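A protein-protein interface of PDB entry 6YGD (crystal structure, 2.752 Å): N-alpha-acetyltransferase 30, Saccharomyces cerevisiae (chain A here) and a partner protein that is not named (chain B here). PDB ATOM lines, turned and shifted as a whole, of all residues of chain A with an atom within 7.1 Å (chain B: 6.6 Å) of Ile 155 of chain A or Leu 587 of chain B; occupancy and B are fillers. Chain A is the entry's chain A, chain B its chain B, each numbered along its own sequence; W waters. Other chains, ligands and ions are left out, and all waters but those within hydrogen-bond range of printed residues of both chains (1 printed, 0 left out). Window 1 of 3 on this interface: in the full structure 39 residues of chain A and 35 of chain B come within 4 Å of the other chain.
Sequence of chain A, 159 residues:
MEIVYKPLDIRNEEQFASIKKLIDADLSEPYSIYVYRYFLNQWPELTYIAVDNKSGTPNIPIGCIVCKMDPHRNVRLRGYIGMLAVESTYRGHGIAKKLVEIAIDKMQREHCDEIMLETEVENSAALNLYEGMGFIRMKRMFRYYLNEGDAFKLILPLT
Printed residues of chain B within 4 Å of Gly 134 of chain A: Ile 584.
Of the printed residues of chain B, Met 138 of chain A touches Leu 587.
Of chain B, only Leu 587 (3.6 Å) comes within 4 Å of Ile 155 of chain A.
Of the printed residues of chain B, Leu 158 of chain A touches Leu 583 (3.4 Å).
Leu 587 of chain B touches four residues of chain A.
The nearest residue of chain A that does not touch Leu 587 of chain B is Leu 156 of chain A (4.9 Å).
Water W1 lies within hydrogen-bond range of NH2 of Arg 588 of chain B and N of Arg 137 of chain A.
CD1 of Ile 584 of chain B touches O of Gly 134 of chain A, 3.5 Å away.
CG2 of Ile 136 of chain A touches CG2 of Ile 584 of chain B, at 3.7 Å.
Leu 587 of chain B touches Ile 136 of chain A (CD2 to CD1, 3.8 Å).
Ile 136 of chain A touches Arg 588 of chain B (CB to NH2, 3.6 Å).
Leu 587 of chain B touches Ile 155 of chain A.
Leu 583 of chain B touches Pro 157 of chain A (O to CG, 3.7 Å).
Ile 584 of chain B touches Pro 157 of chain A (CA to CG, 3.9 Å).
Pro 157 of chain A touches Leu 587 of chain B.
O of Leu 158 of chain A touches CD1 of Leu 583 of chain B, 3.4 Å away.
Of the 10 printed residues of chain B, 4 touch a printed residue of chain A.
Hydrophobic or aromatic side chains of chain B that line the printed part of chain A: Leu 583, Ile 584 and Leu 587.
Hydrophobic or aromatic side chains of chain A within 4 Å of the printed part of chain B: Ile 136, Met 138, Ile 155 and Pro 157.
Among the printed residues, no Asp or Glu carboxylate lies within 4 Å of a Lys or Arg side-chain nitrogen of the other chain.
The guanidinium group (NH2) of Arg 588 of chain B lies within hydrogen-bond range of the backbone carbonyl oxygen (O) of Arg 137 of chain A (2.7 Å).
The side-chain sulfur of Met 138 of chain A sits close to the backbone carbonyl oxygen of Leu 587 of chain B, 3.8 Å away.
O of Asp 113 of chain A sits at hydrogen-bond distance from N of Leu 158 of chain A (2.8 Å).
The backbone carbonyl oxygen of Ile 136 of chain A is in hydrogen-bond range of the backbone NH of Ile 155 of chain A, 3.1 Å away.
The backbone NH of Met 138 of chain A lies within hydrogen-bond range of the backbone carbonyl oxygen of Lys 153 of chain A, 2.9 Å away.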
ATOM      1  N   HIS A  72      26.946 -32.777  32.692  1.00  0.00           N
ATOM      2  CA  HIS A  72      28.345 -32.450  32.482  1.00  0.00           C
ATOM      3  C   HIS A  72      28.935 -32.021  33.816  1.00  0.00           C
ATOM      4  O   HIS A  72      28.320 -31.235  34.547  1.00  0.00           O
ATOM      5  CB  HIS A  72      28.522 -31.341  31.444  1.00  0.00           C
ATOM      6  CG  HIS A  72      29.948 -31.117  31.059  1.00  0.00           C
ATOM      7  ND1 HIS A  72      30.643 -29.976  31.399  1.00  0.00           N
ATOM      8  CD2 HIS A  72      30.824 -31.909  30.397  1.00  0.00           C
ATOM      9  CE1 HIS A  72      31.881 -30.067  30.946  1.00  0.00           C
ATOM     10  NE2 HIS A  72      32.017 -31.232  30.338  1.00  0.00           N
ATOM     11  N   ARG A  76      25.694 -29.347  35.924  1.00  0.00           N
ATOM     12  CA  ARG A  76      25.067 -28.831  34.716  1.00  0.00           C
ATOM     13  C   ARG A  76      24.617 -29.977  33.825  1.00  0.00           C
ATOM     14  O   ARG A  76      25.259 -31.030  33.783  1.00  0.00           O
ATOM     15  CB  ARG A  76      26.014 -27.891  33.955  1.00  0.00           C
ATOM     16  CG  ARG A  76      26.338 -26.618  34.727  1.00  0.00           C
ATOM     17  CD  ARG A  76      27.321 -25.725  34.005  1.00  0.00           C
ATOM     18  NE  ARG A  76      26.778 -25.173  32.769  1.00  0.00           N
ATOM     19  CZ  ARG A  76      25.932 -24.148  32.711  1.00  0.00           C
ATOM     20  NH1 ARG A  76      25.513 -23.566  33.825  1.00  0.00           N
ATOM     21  NH2 ARG A  76      25.500 -23.704  31.537  1.00  0.00           N
ATOM     22  N   ARG A  78      24.086 -31.101  30.033  1.00  0.00           N
ATOM     23  CA  ARG A  78      24.650 -30.758  28.735  1.00  0.00           C
ATOM     24  C   ARG A  78      23.929 -31.533  27.643  1.00  0.00           C
ATOM     25  O   ARG A  78      24.081 -32.755  27.532  1.00  0.00           O
ATOM     26  CB  ARG A  78      26.146 -31.047  28.704  1.00  0.00           C
ATOM     27  CG  ARG A  78      26.739 -30.991  27.327  1.00  0.00           C
ATOM     28  CD  ARG A  78      28.227 -31.209  27.366  1.00  0.00           C
ATOM     29  NE  ARG A  78      28.929 -29.981  27.711  1.00  0.00           N
ATOM     30  CZ  ARG A  78      30.242 -29.814  27.597  1.00  0.00           C
ATOM     31  NH1 ARG A  78      31.006 -30.799  27.146  1.00  0.00           N
ATOM     32  NH2 ARG A  78      30.792 -28.659  27.938  1.00  0.00           N
ATOM     33  N   ASP A 113      21.387 -26.995  30.394  1.00  0.00           N
ATOM     34  CA  ASP A 113      22.076 -25.733  30.601  1.00  0.00           C
ATOM     35  C   ASP A 113      22.884 -25.296  29.390  1.00  0.00           C
ATOM     36  O   ASP A 113      23.156 -24.101  29.240  1.00  0.00           O
ATOM     37  CB  ASP A 113      23.002 -25.843  31.813  1.00  0.00           C
ATOM     38  CG  ASP A 113      22.253 -26.175  33.082  1.00  0.00           C
ATOM     39  OD1 ASP A 113      21.167 -25.597  33.297  1.00  0.00           O
ATOM     40  OD2 ASP A 113      22.741 -27.022  33.856  1.00  0.00           O
ATOM     41  N   GLU A 114      23.266 -26.233  28.526  1.00  0.00           N
ATOM     42  CA  GLU A 114      24.061 -25.910  27.354  1.00  0.00           C
ATOM     43  C   GLU A 114      23.846 -26.981  26.294  1.00  0.00           C
ATOM     44  O   GLU A 114      23.395 -28.090  26.586  1.00  0.00           O
ATOM     45  CB  GLU A 114      25.543 -25.793  27.711  1.00  0.00           C
ATOM     46  CG  GLU A 114      26.149 -27.087  28.222  1.00  0.00           C
ATOM     47  CD  GLU A 114      27.477 -26.865  28.913  1.00  0.00           C
ATOM     48  OE1 GLU A 114      27.610 -25.846  29.626  1.00  0.00           O
ATOM     49  OE2 GLU A 114      28.389 -27.701  28.736  1.00  0.00           O
ATOM     50  N   ILE A 115      24.169 -26.625  25.053  1.00  0.00           N
ATOM     51  CA  ILE A 115      24.120 -27.548  23.926  1.00  0.00           C
ATOM     52  C   ILE A 115      25.512 -27.632  23.323  1.00  0.00           C
ATOM     53  O   ILE A 115      26.180 -26.610  23.144  1.00  0.00           O
ATOM     54  CB  ILE A 115      23.096 -27.112  22.862  1.00  0.00           C
ATOM     55  CG1 ILE A 115      21.757 -26.787  23.514  1.00  0.00           C
ATOM     56  CG2 ILE A 115      22.908 -28.213  21.833  1.00  0.00           C
ATOM     57  CD1 ILE A 115      21.102 -27.984  24.153  1.00  0.00           C
ATOM     58  N   MET A 116      25.947 -28.841  23.006  1.00  0.00           N
ATOM     59  CA  MET A 116      27.293 -29.058  22.501  1.00  0.00           C
ATOM     60  C   MET A 116      27.247 -29.925  21.252  1.00  0.00           C
ATOM     61  O   MET A 116      26.399 -30.809  21.123  1.00  0.00           O
ATOM     62  CB  MET A 116      28.173 -29.714  23.565  1.00  0.00           C
ATOM     63  CG  MET A 116      29.666 -29.540  23.350  1.00  0.00           C
ATOM     64  SD  MET A 116      30.424 -30.940  22.514  1.00  0.00           S
ATOM     65  CE  MET A 116      30.107 -32.245  23.701  1.00  0.00           C
ATOM     66  N   LEU A 117      28.171 -29.661  20.334  1.00  0.00           N
ATOM     67  CA  LEU A 117      28.301 -30.484  19.140  1.00  0.00           C
ATOM     68  C   LEU A 117      29.696 -30.289  18.569  1.00  0.00           C
ATOM     69  O   LEU A 117      30.389 -29.324  18.896  1.00  0.00           O
ATOM     70  CB  LEU A 117      27.226 -30.141  18.105  1.00  0.00           C
ATOM     71  CG  LEU A 117      27.449 -28.877  17.280  1.00  0.00           C
ATOM     72  CD1 LEU A 117      27.881 -29.277  15.885  1.00  0.00           C
ATOM     73  CD2 LEU A 117      26.190 -28.024  17.238  1.00  0.00           C
ATOM     74  N   GLY A 134      23.338 -18.656  17.823  1.00  0.00           N
ATOM     75  CA  GLY A 134      23.995 -18.285  19.059  1.00  0.00           C
ATOM     76  C   GLY A 134      25.176 -19.153  19.429  1.00  0.00           C
ATOM     77  O   GLY A 134      25.869 -18.833  20.401  1.00  0.00           O
ATOM     78  N   PHE A 135      25.425 -20.238  18.699  1.00  0.00           N
ATOM     79  CA  PHE A 135      26.572 -21.092  18.986  1.00  0.00           C
ATOM     80  C   PHE A 135      27.870 -20.330  18.756  1.00  0.00           C
ATOM     81  O   PHE A 135      27.994 -19.557  17.802  1.00  0.00           O
ATOM     82  CB  PHE A 135      26.554 -22.339  18.095  1.00  0.00           C
ATOM     83  CG  PHE A 135      25.685 -23.462  18.603  1.00  0.00           C
ATOM     84  CD1 PHE A 135      24.353 -23.552  18.232  1.00  0.00           C
ATOM     85  CD2 PHE A 135      26.214 -24.451  19.417  1.00  0.00           C
ATOM     86  CE1 PHE A 135      23.560 -24.595  18.679  1.00  0.00           C
ATOM     87  CE2 PHE A 135      25.426 -25.495  19.871  1.00  0.00           C
ATOM     88  CZ  PHE A 135      24.097 -25.567  19.500  1.00  0.00           C
ATOM     89  N   ILE A 136      28.847 -20.555  19.632  1.00  0.00           N
ATOM     90  CA  ILE A 136      30.191 -20.033  19.434  1.00  0.00           C
ATOM     91  C   ILE A 136      31.175 -21.192  19.490  1.00  0.00           C
ATOM     92  O   ILE A 136      30.857 -22.294  19.945  1.00  0.00           O
ATOM     93  CB  ILE A 136      30.579 -18.950  20.464  1.00  0.00           C
ATOM     94  CG1 ILE A 136      30.425 -19.477  21.890  1.00  0.00           C
ATOM     95  CG2 ILE A 136      29.769 -17.680  20.241  1.00  0.00           C
ATOM     96  CD1 ILE A 136      30.983 -18.544  22.944  1.00  0.00           C
ATOM     97  N   ARG A 137      32.386 -20.931  19.012  1.00  0.00           N
ATOM     98  CA  ARG A 137      33.437 -21.936  18.988  1.00  0.00           C
ATOM     99  C   ARG A 137      34.249 -21.853  20.271  1.00  0.00           C
ATOM    100  O   ARG A 137      34.746 -20.781  20.630  1.00  0.00           O
ATOM    101  CB  ARG A 137      34.337 -21.738  17.771  1.00  0.00           C
ATOM    102  CG  ARG A 137      33.565 -21.602  16.480  1.00  0.00           C
ATOM    103  CD  ARG A 137      34.477 -21.224  15.342  1.00  0.00           C
ATOM    104  NE  ARG A 137      33.727 -20.976  14.117  1.00  0.00           N
ATOM    105  CZ  ARG A 137      34.231 -20.363  13.052  1.00  0.00           C
ATOM    106  NH1 ARG A 137      35.486 -19.935  13.069  1.00  0.00           N
ATOM    107  NH2 ARG A 137      33.482 -20.176  11.975  1.00  0.00           N
ATOM    108  N   MET A 138      34.375 -22.983  20.961  1.00  0.00           N
ATOM    109  CA  MET A 138      35.104 -23.044  22.217  1.00  0.00           C
ATOM    110  C   MET A 138      36.400 -23.835  22.128  1.00  0.00           C
ATOM    111  O   MET A 138      37.195 -23.796  23.075  1.00  0.00           O
ATOM    112  CB  MET A 138      34.217 -23.652  23.316  1.00  0.00           C
ATOM    113  CG  MET A 138      32.959 -22.843  23.646  1.00  0.00           C
ATOM    114  SD  MET A 138      33.290 -21.212  24.361  1.00  0.00           S
ATOM    115  CE  MET A 138      34.298 -21.643  25.779  1.00  0.00           C
ATOM    116  N   LYS A 153      34.459 -27.314  18.301  1.00  0.00           N
ATOM    117  CA  LYS A 153      33.512 -27.698  19.336  1.00  0.00           C
ATOM    118  C   LYS A 153      32.613 -26.496  19.592  1.00  0.00           C
ATOM    119  O   LYS A 153      33.080 -25.457  20.067  1.00  0.00           O
ATOM    120  CB  LYS A 153      34.260 -28.139  20.592  1.00  0.00           C
ATOM    121  CG  LYS A 153      33.401 -28.494  21.790  1.00  0.00           C
ATOM    122  CD  LYS A 153      34.274 -29.051  22.907  1.00  0.00           C
ATOM    123  CE  LYS A 153      33.448 -29.484  24.111  1.00  0.00           C
ATOM    124  NZ  LYS A 153      34.287 -30.041  25.216  1.00  0.00           N
ATOM    125  N   LEU A 154      31.340 -26.616  19.238  1.00  0.00           N
ATOM    126  CA  LEU A 154      30.390 -25.521  19.367  1.00  0.00           C
ATOM    127  C   LEU A 154      29.555 -25.716  20.620  1.00  0.00           C
ATOM    128  O   LEU A 154      29.089 -26.827  20.892  1.00  0.00           O
ATOM    129  CB  LEU A 154      29.476 -25.437  18.146  1.00  0.00           C
ATOM    130  CG  LEU A 154      30.128 -25.430  16.765  1.00  0.00           C
ATOM    131  CD1 LEU A 154      29.070 -25.199  15.699  1.00  0.00           C
ATOM    132  CD2 LEU A 154      31.231 -24.393  16.659  1.00  0.00           C
ATOM    133  N   ILE A 155      29.365 -24.639  21.374  1.00  0.00           N
ATOM    134  CA  ILE A 155      28.566 -24.670  22.590  1.00  0.00           C
ATOM    135  C   ILE A 155      27.575 -23.520  22.549  1.00  0.00           C
ATOM    136  O   ILE A 155      27.936 -22.394  22.190  1.00  0.00           O
ATOM    137  CB  ILE A 155      29.428 -24.594  23.864  1.00  0.00           C
ATOM    138  CG1 ILE A 155      30.281 -25.850  24.014  1.00  0.00           C
ATOM    139  CG2 ILE A 155      28.546 -24.463  25.087  1.00  0.00           C
ATOM    140  CD1 ILE A 155      30.914 -25.974  25.384  1.00  0.00           C
ATOM    141  N   LEU A 156      26.329 -23.811  22.903  1.00  0.00           N
ATOM    142  CA  LEU A 156      25.286 -22.804  23.023  1.00  0.00           C
ATOM    143  C   LEU A 156      24.827 -22.742  24.471  1.00  0.00           C
ATOM    144  O   LEU A 156      24.220 -23.707  24.958  1.00  0.00           O
ATOM    145  CB  LEU A 156      24.113 -23.136  22.103  1.00  0.00           C
ATOM    146  CG  LEU A 156      22.870 -22.255  22.206  1.00  0.00           C
ATOM    147  CD1 LEU A 156      23.177 -20.819  21.795  1.00  0.00           C
ATOM    148  CD2 LEU A 156      21.747 -22.833  21.355  1.00  0.00           C
ATOM    149  N   PRO A 157      25.069 -21.644  25.190  1.00  0.00           N
ATOM    150  CA  PRO A 157      24.703 -21.576  26.615  1.00  0.00           C
ATOM    151  C   PRO A 157      23.251 -21.160  26.795  1.00  0.00           C
ATOM    152  O   PRO A 157      22.831 -20.107  26.312  1.00  0.00           O
ATOM    153  CB  PRO A 157      25.665 -20.522  27.175  1.00  0.00           C
ATOM    154  CG  PRO A 157      26.052 -19.673  25.963  1.00  0.00           C
ATOM    155  CD  PRO A 157      25.615 -20.371  24.700  1.00  0.00           C
ATOM    156  N   LEU A 158      22.487 -21.985  27.511  1.00  0.00           N
ATOM    157  CA  LEU A 158      21.078 -21.733  27.790  1.00  0.00           C
ATOM    158  C   LEU A 158      20.840 -21.142  29.169  1.00  0.00           C
ATOM    159  O   LEU A 158      19.902 -20.357  29.339  1.00  0.00           O
ATOM    160  CB  LEU A 158      20.271 -23.032  27.667  1.00  0.00           C
ATOM    161  CG  LEU A 158      20.264 -23.754  26.317  1.00  0.00           C
ATOM    162  CD1 LEU A 158      19.358 -24.967  26.372  1.00  0.00           C
ATOM    163  CD2 LEU A 158      19.837 -22.808  25.204  1.00  0.00           C
ATOM    164  N   ARG B 582      24.497 -11.826  26.932  1.00  0.00           N
ATOM    165  CA  ARG B 582      25.290 -11.906  28.156  1.00  0.00           C
ATOM    166  C   ARG B 582      25.754 -13.332  28.428  1.00  0.00           C
ATOM    167  O   ARG B 582      26.915 -13.552  28.789  1.00  0.00           O
ATOM    168  CB  ARG B 582      24.493 -11.369  29.344  1.00  0.00           C
ATOM    169  CG  ARG B 582      25.261 -11.382  30.659  1.00  0.00           C
ATOM    170  CD  ARG B 582      24.375 -10.989  31.831  1.00  0.00           C
ATOM    171  NE  ARG B 582      23.957  -9.590  31.767  1.00  0.00           N
ATOM    172  CZ  ARG B 582      24.448  -8.629  32.544  1.00  0.00           C
ATOM    173  NH1 ARG B 582      25.373  -8.915  33.450  1.00  0.00           N
ATOM    174  NH2 ARG B 582      24.012  -7.384  32.416  1.00  0.00           N
ATOM    175  N   LEU B 583      24.861 -14.312  28.261  1.00  0.00           N
ATOM    176  CA  LEU B 583      25.250 -15.705  28.459  1.00  0.00           C
ATOM    177  C   LEU B 583      26.352 -16.112  27.494  1.00  0.00           C
ATOM    178  O   LEU B 583      27.313 -16.789  27.884  1.00  0.00           O
ATOM    179  CB  LEU B 583      24.040 -16.622  28.295  1.00  0.00           C
ATOM    180  CG  LEU B 583      23.090 -16.722  29.485  1.00  0.00           C
ATOM    181  CD1 LEU B 583      21.995 -17.725  29.184  1.00  0.00           C
ATOM    182  CD2 LEU B 583      23.854 -17.111  30.742  1.00  0.00           C
ATOM    183  N   ILE B 584      26.228 -15.713  26.227  1.00  0.00           N
ATOM    184  CA  ILE B 584      27.257 -16.026  25.241  1.00  0.00           C
ATOM    185  C   ILE B 584      28.574 -15.371  25.630  1.00  0.00           C
ATOM    186  O   ILE B 584      29.646 -15.976  25.511  1.00  0.00           O
ATOM    187  CB  ILE B 584      26.797 -15.593  23.835  1.00  0.00           C
ATOM    188  CG1 ILE B 584      25.564 -16.395  23.410  1.00  0.00           C
ATOM    189  CG2 ILE B 584      27.927 -15.751  22.824  1.00  0.00           C
ATOM    190  CD1 ILE B 584      24.964 -15.946  22.101  1.00  0.00           C
ATOM    191  N   HIS B 585      28.508 -14.132  26.119  1.00  0.00           N
ATOM    192  CA  HIS B 585      29.717 -13.426  26.529  1.00  0.00           C
ATOM    193  C   HIS B 585      30.388 -14.108  27.713  1.00  0.00           C
ATOM    194  O   HIS B 585      31.615 -14.259  27.735  1.00  0.00           O
ATOM    195  CB  HIS B 585      29.388 -11.976  26.875  1.00  0.00           C
ATOM    196  CG  HIS B 585      30.549 -11.223  27.441  1.00  0.00           C
ATOM    197  ND1 HIS B 585      30.820 -11.179  28.792  1.00  0.00           N
ATOM    198  CD2 HIS B 585      31.522 -10.501  26.837  1.00  0.00           C
ATOM    199  CE1 HIS B 585      31.905 -10.454  28.996  1.00  0.00           C
ATOM    200  NE2 HIS B 585      32.352 -10.033  27.827  1.00  0.00           N
ATOM    201  N   ASN B 586      29.603 -14.516  28.715  1.00  0.00           N
ATOM    202  CA  ASN B 586      30.187 -15.176  29.876  1.00  0.00           C
ATOM    203  C   ASN B 586      30.795 -16.521  29.508  1.00  0.00           C
ATOM    204  O   ASN B 586      31.763 -16.954  30.145  1.00  0.00           O
ATOM    205  CB  ASN B 586      29.140 -15.353  30.973  1.00  0.00           C
ATOM    206  CG  ASN B 586      28.620 -14.032  31.500  1.00  0.00           C
ATOM    207  OD1 ASN B 586      29.250 -12.986  31.326  1.00  0.00           O
ATOM    208  ND2 ASN B 586      27.463 -14.071  32.148  1.00  0.00           N
ATOM    209  N   LEU B 587      30.246 -17.192  28.494  1.00  0.00           N
ATOM    210  CA  LEU B 587      30.815 -18.462  28.056  1.00  0.00           C
ATOM    211  C   LEU B 587      32.145 -18.253  27.342  1.00  0.00           C
ATOM    212  O   LEU B 587      33.059 -19.077  27.469  1.00  0.00           O
ATOM    213  CB  LEU B 587      29.822 -19.198  27.154  1.00  0.00           C
ATOM    214  CG  LEU B 587      30.355 -20.449  26.451  1.00  0.00           C
ATOM    215  CD1 LEU B 587      30.679 -21.547  27.460  1.00  0.00           C
ATOM    216  CD2 LEU B 587      29.378 -20.943  25.402  1.00  0.00           C
ATOM    217  N   ARG B 588      32.273 -17.154  26.597  1.00  0.00           N
ATOM    218  CA  ARG B 588      33.522 -16.858  25.899  1.00  0.00           C
ATOM    219  C   ARG B 588      34.656 -16.575  26.879  1.00  0.00           C
ATOM    220  O   ARG B 588      35.779 -17.058  26.692  1.00  0.00           O
ATOM    221  CB  ARG B 588      33.310 -15.679  24.945  1.00  0.00           C
ATOM    222  CG  ARG B 588      34.572 -15.146  24.277  1.00  0.00           C
ATOM    223  CD  ARG B 588      35.318 -16.233  23.519  1.00  0.00           C
ATOM    224  NE  ARG B 588      34.595 -16.695  22.341  1.00  0.00           N
ATOM    225  CZ  ARG B 588      34.835 -17.848  21.727  1.00  0.00           C
ATOM    226  NH1 ARG B 588      35.776 -18.660  22.186  1.00  0.00           N
ATOM    227  NH2 ARG B 588      34.131 -18.198  20.660  1.00  0.00           N
ATOM    228  N   PHE B 589      34.387 -15.802  27.931  1.00  0.00           N
ATOM    229  CA  PHE B 589      35.397 -15.459  28.924  1.00  0.00           C
ATOM    230  C   PHE B 589      35.345 -16.362  30.150  1.00  0.00           C
ATOM    231  O   PHE B 589      35.883 -16.001  31.201  1.00  0.00           O
ATOM    232  CB  PHE B 589      35.266 -13.990  29.332  1.00  0.00           C
ATOM    233  CG  PHE B 589      35.565 -13.033  28.217  1.00  0.00           C
ATOM    234  CD1 PHE B 589      36.861 -12.613  27.978  1.00  0.00           C
ATOM    235  CD2 PHE B 589      34.554 -12.576  27.389  1.00  0.00           C
ATOM    236  CE1 PHE B 589      37.140 -11.741  26.947  1.00  0.00           C
ATOM    237  CE2 PHE B 589      34.829 -11.704  26.354  1.00  0.00           C
ATOM    238  CZ  PHE B 589      36.123 -11.290  26.132  1.00  0.00           C
ATOM    239  N   LYS B 590      34.716 -17.531  30.026  1.00  0.00           N
ATOM    240  CA  LYS B 590      34.698 -18.495  31.124  1.00  0.00           C
ATOM    241  C   LYS B 590      36.087 -18.905  31.610  1.00  0.00           C
ATOM    242  O   LYS B 590      36.267 -19.007  32.836  1.00  0.00           O
ATOM    243  CB  LYS B 590      33.881 -19.723  30.696  1.00  0.00           C
ATOM    244  CG  LYS B 590      33.901 -20.899  31.669  1.00  0.00           C
ATOM    245  CD  LYS B 590      33.263 -22.136  31.030  1.00  0.00           C
ATOM    246  CE  LYS B 590      33.318 -23.352  31.940  1.00  0.00           C
ATOM    247  NZ  LYS B 590      32.718 -24.552  31.293  1.00  0.00           N
ATOM    248  N   PRO B 591      37.084 -19.161  30.751  1.00  0.00           N
ATOM    249  CA  PRO B 591      38.404 -19.564  31.275  1.00  0.00           C
ATOM    250  C   PRO B 591      39.034 -18.567  32.234  1.00  0.00           C
ATOM    251  O   PRO B 591      39.840 -18.969  33.084  1.00  0.00           O
ATOM    252  CB  PRO B 591      39.246 -19.718  30.001  1.00  0.00           C
ATOM    253  CG  PRO B 591      38.267 -20.076  28.958  1.00  0.00           C
ATOM    254  CD  PRO B 591      37.028 -19.299  29.282  1.00  0.00           C
HETATM  255  O   HOH W   1      33.289 -18.410  18.004  1.00  0.00           O
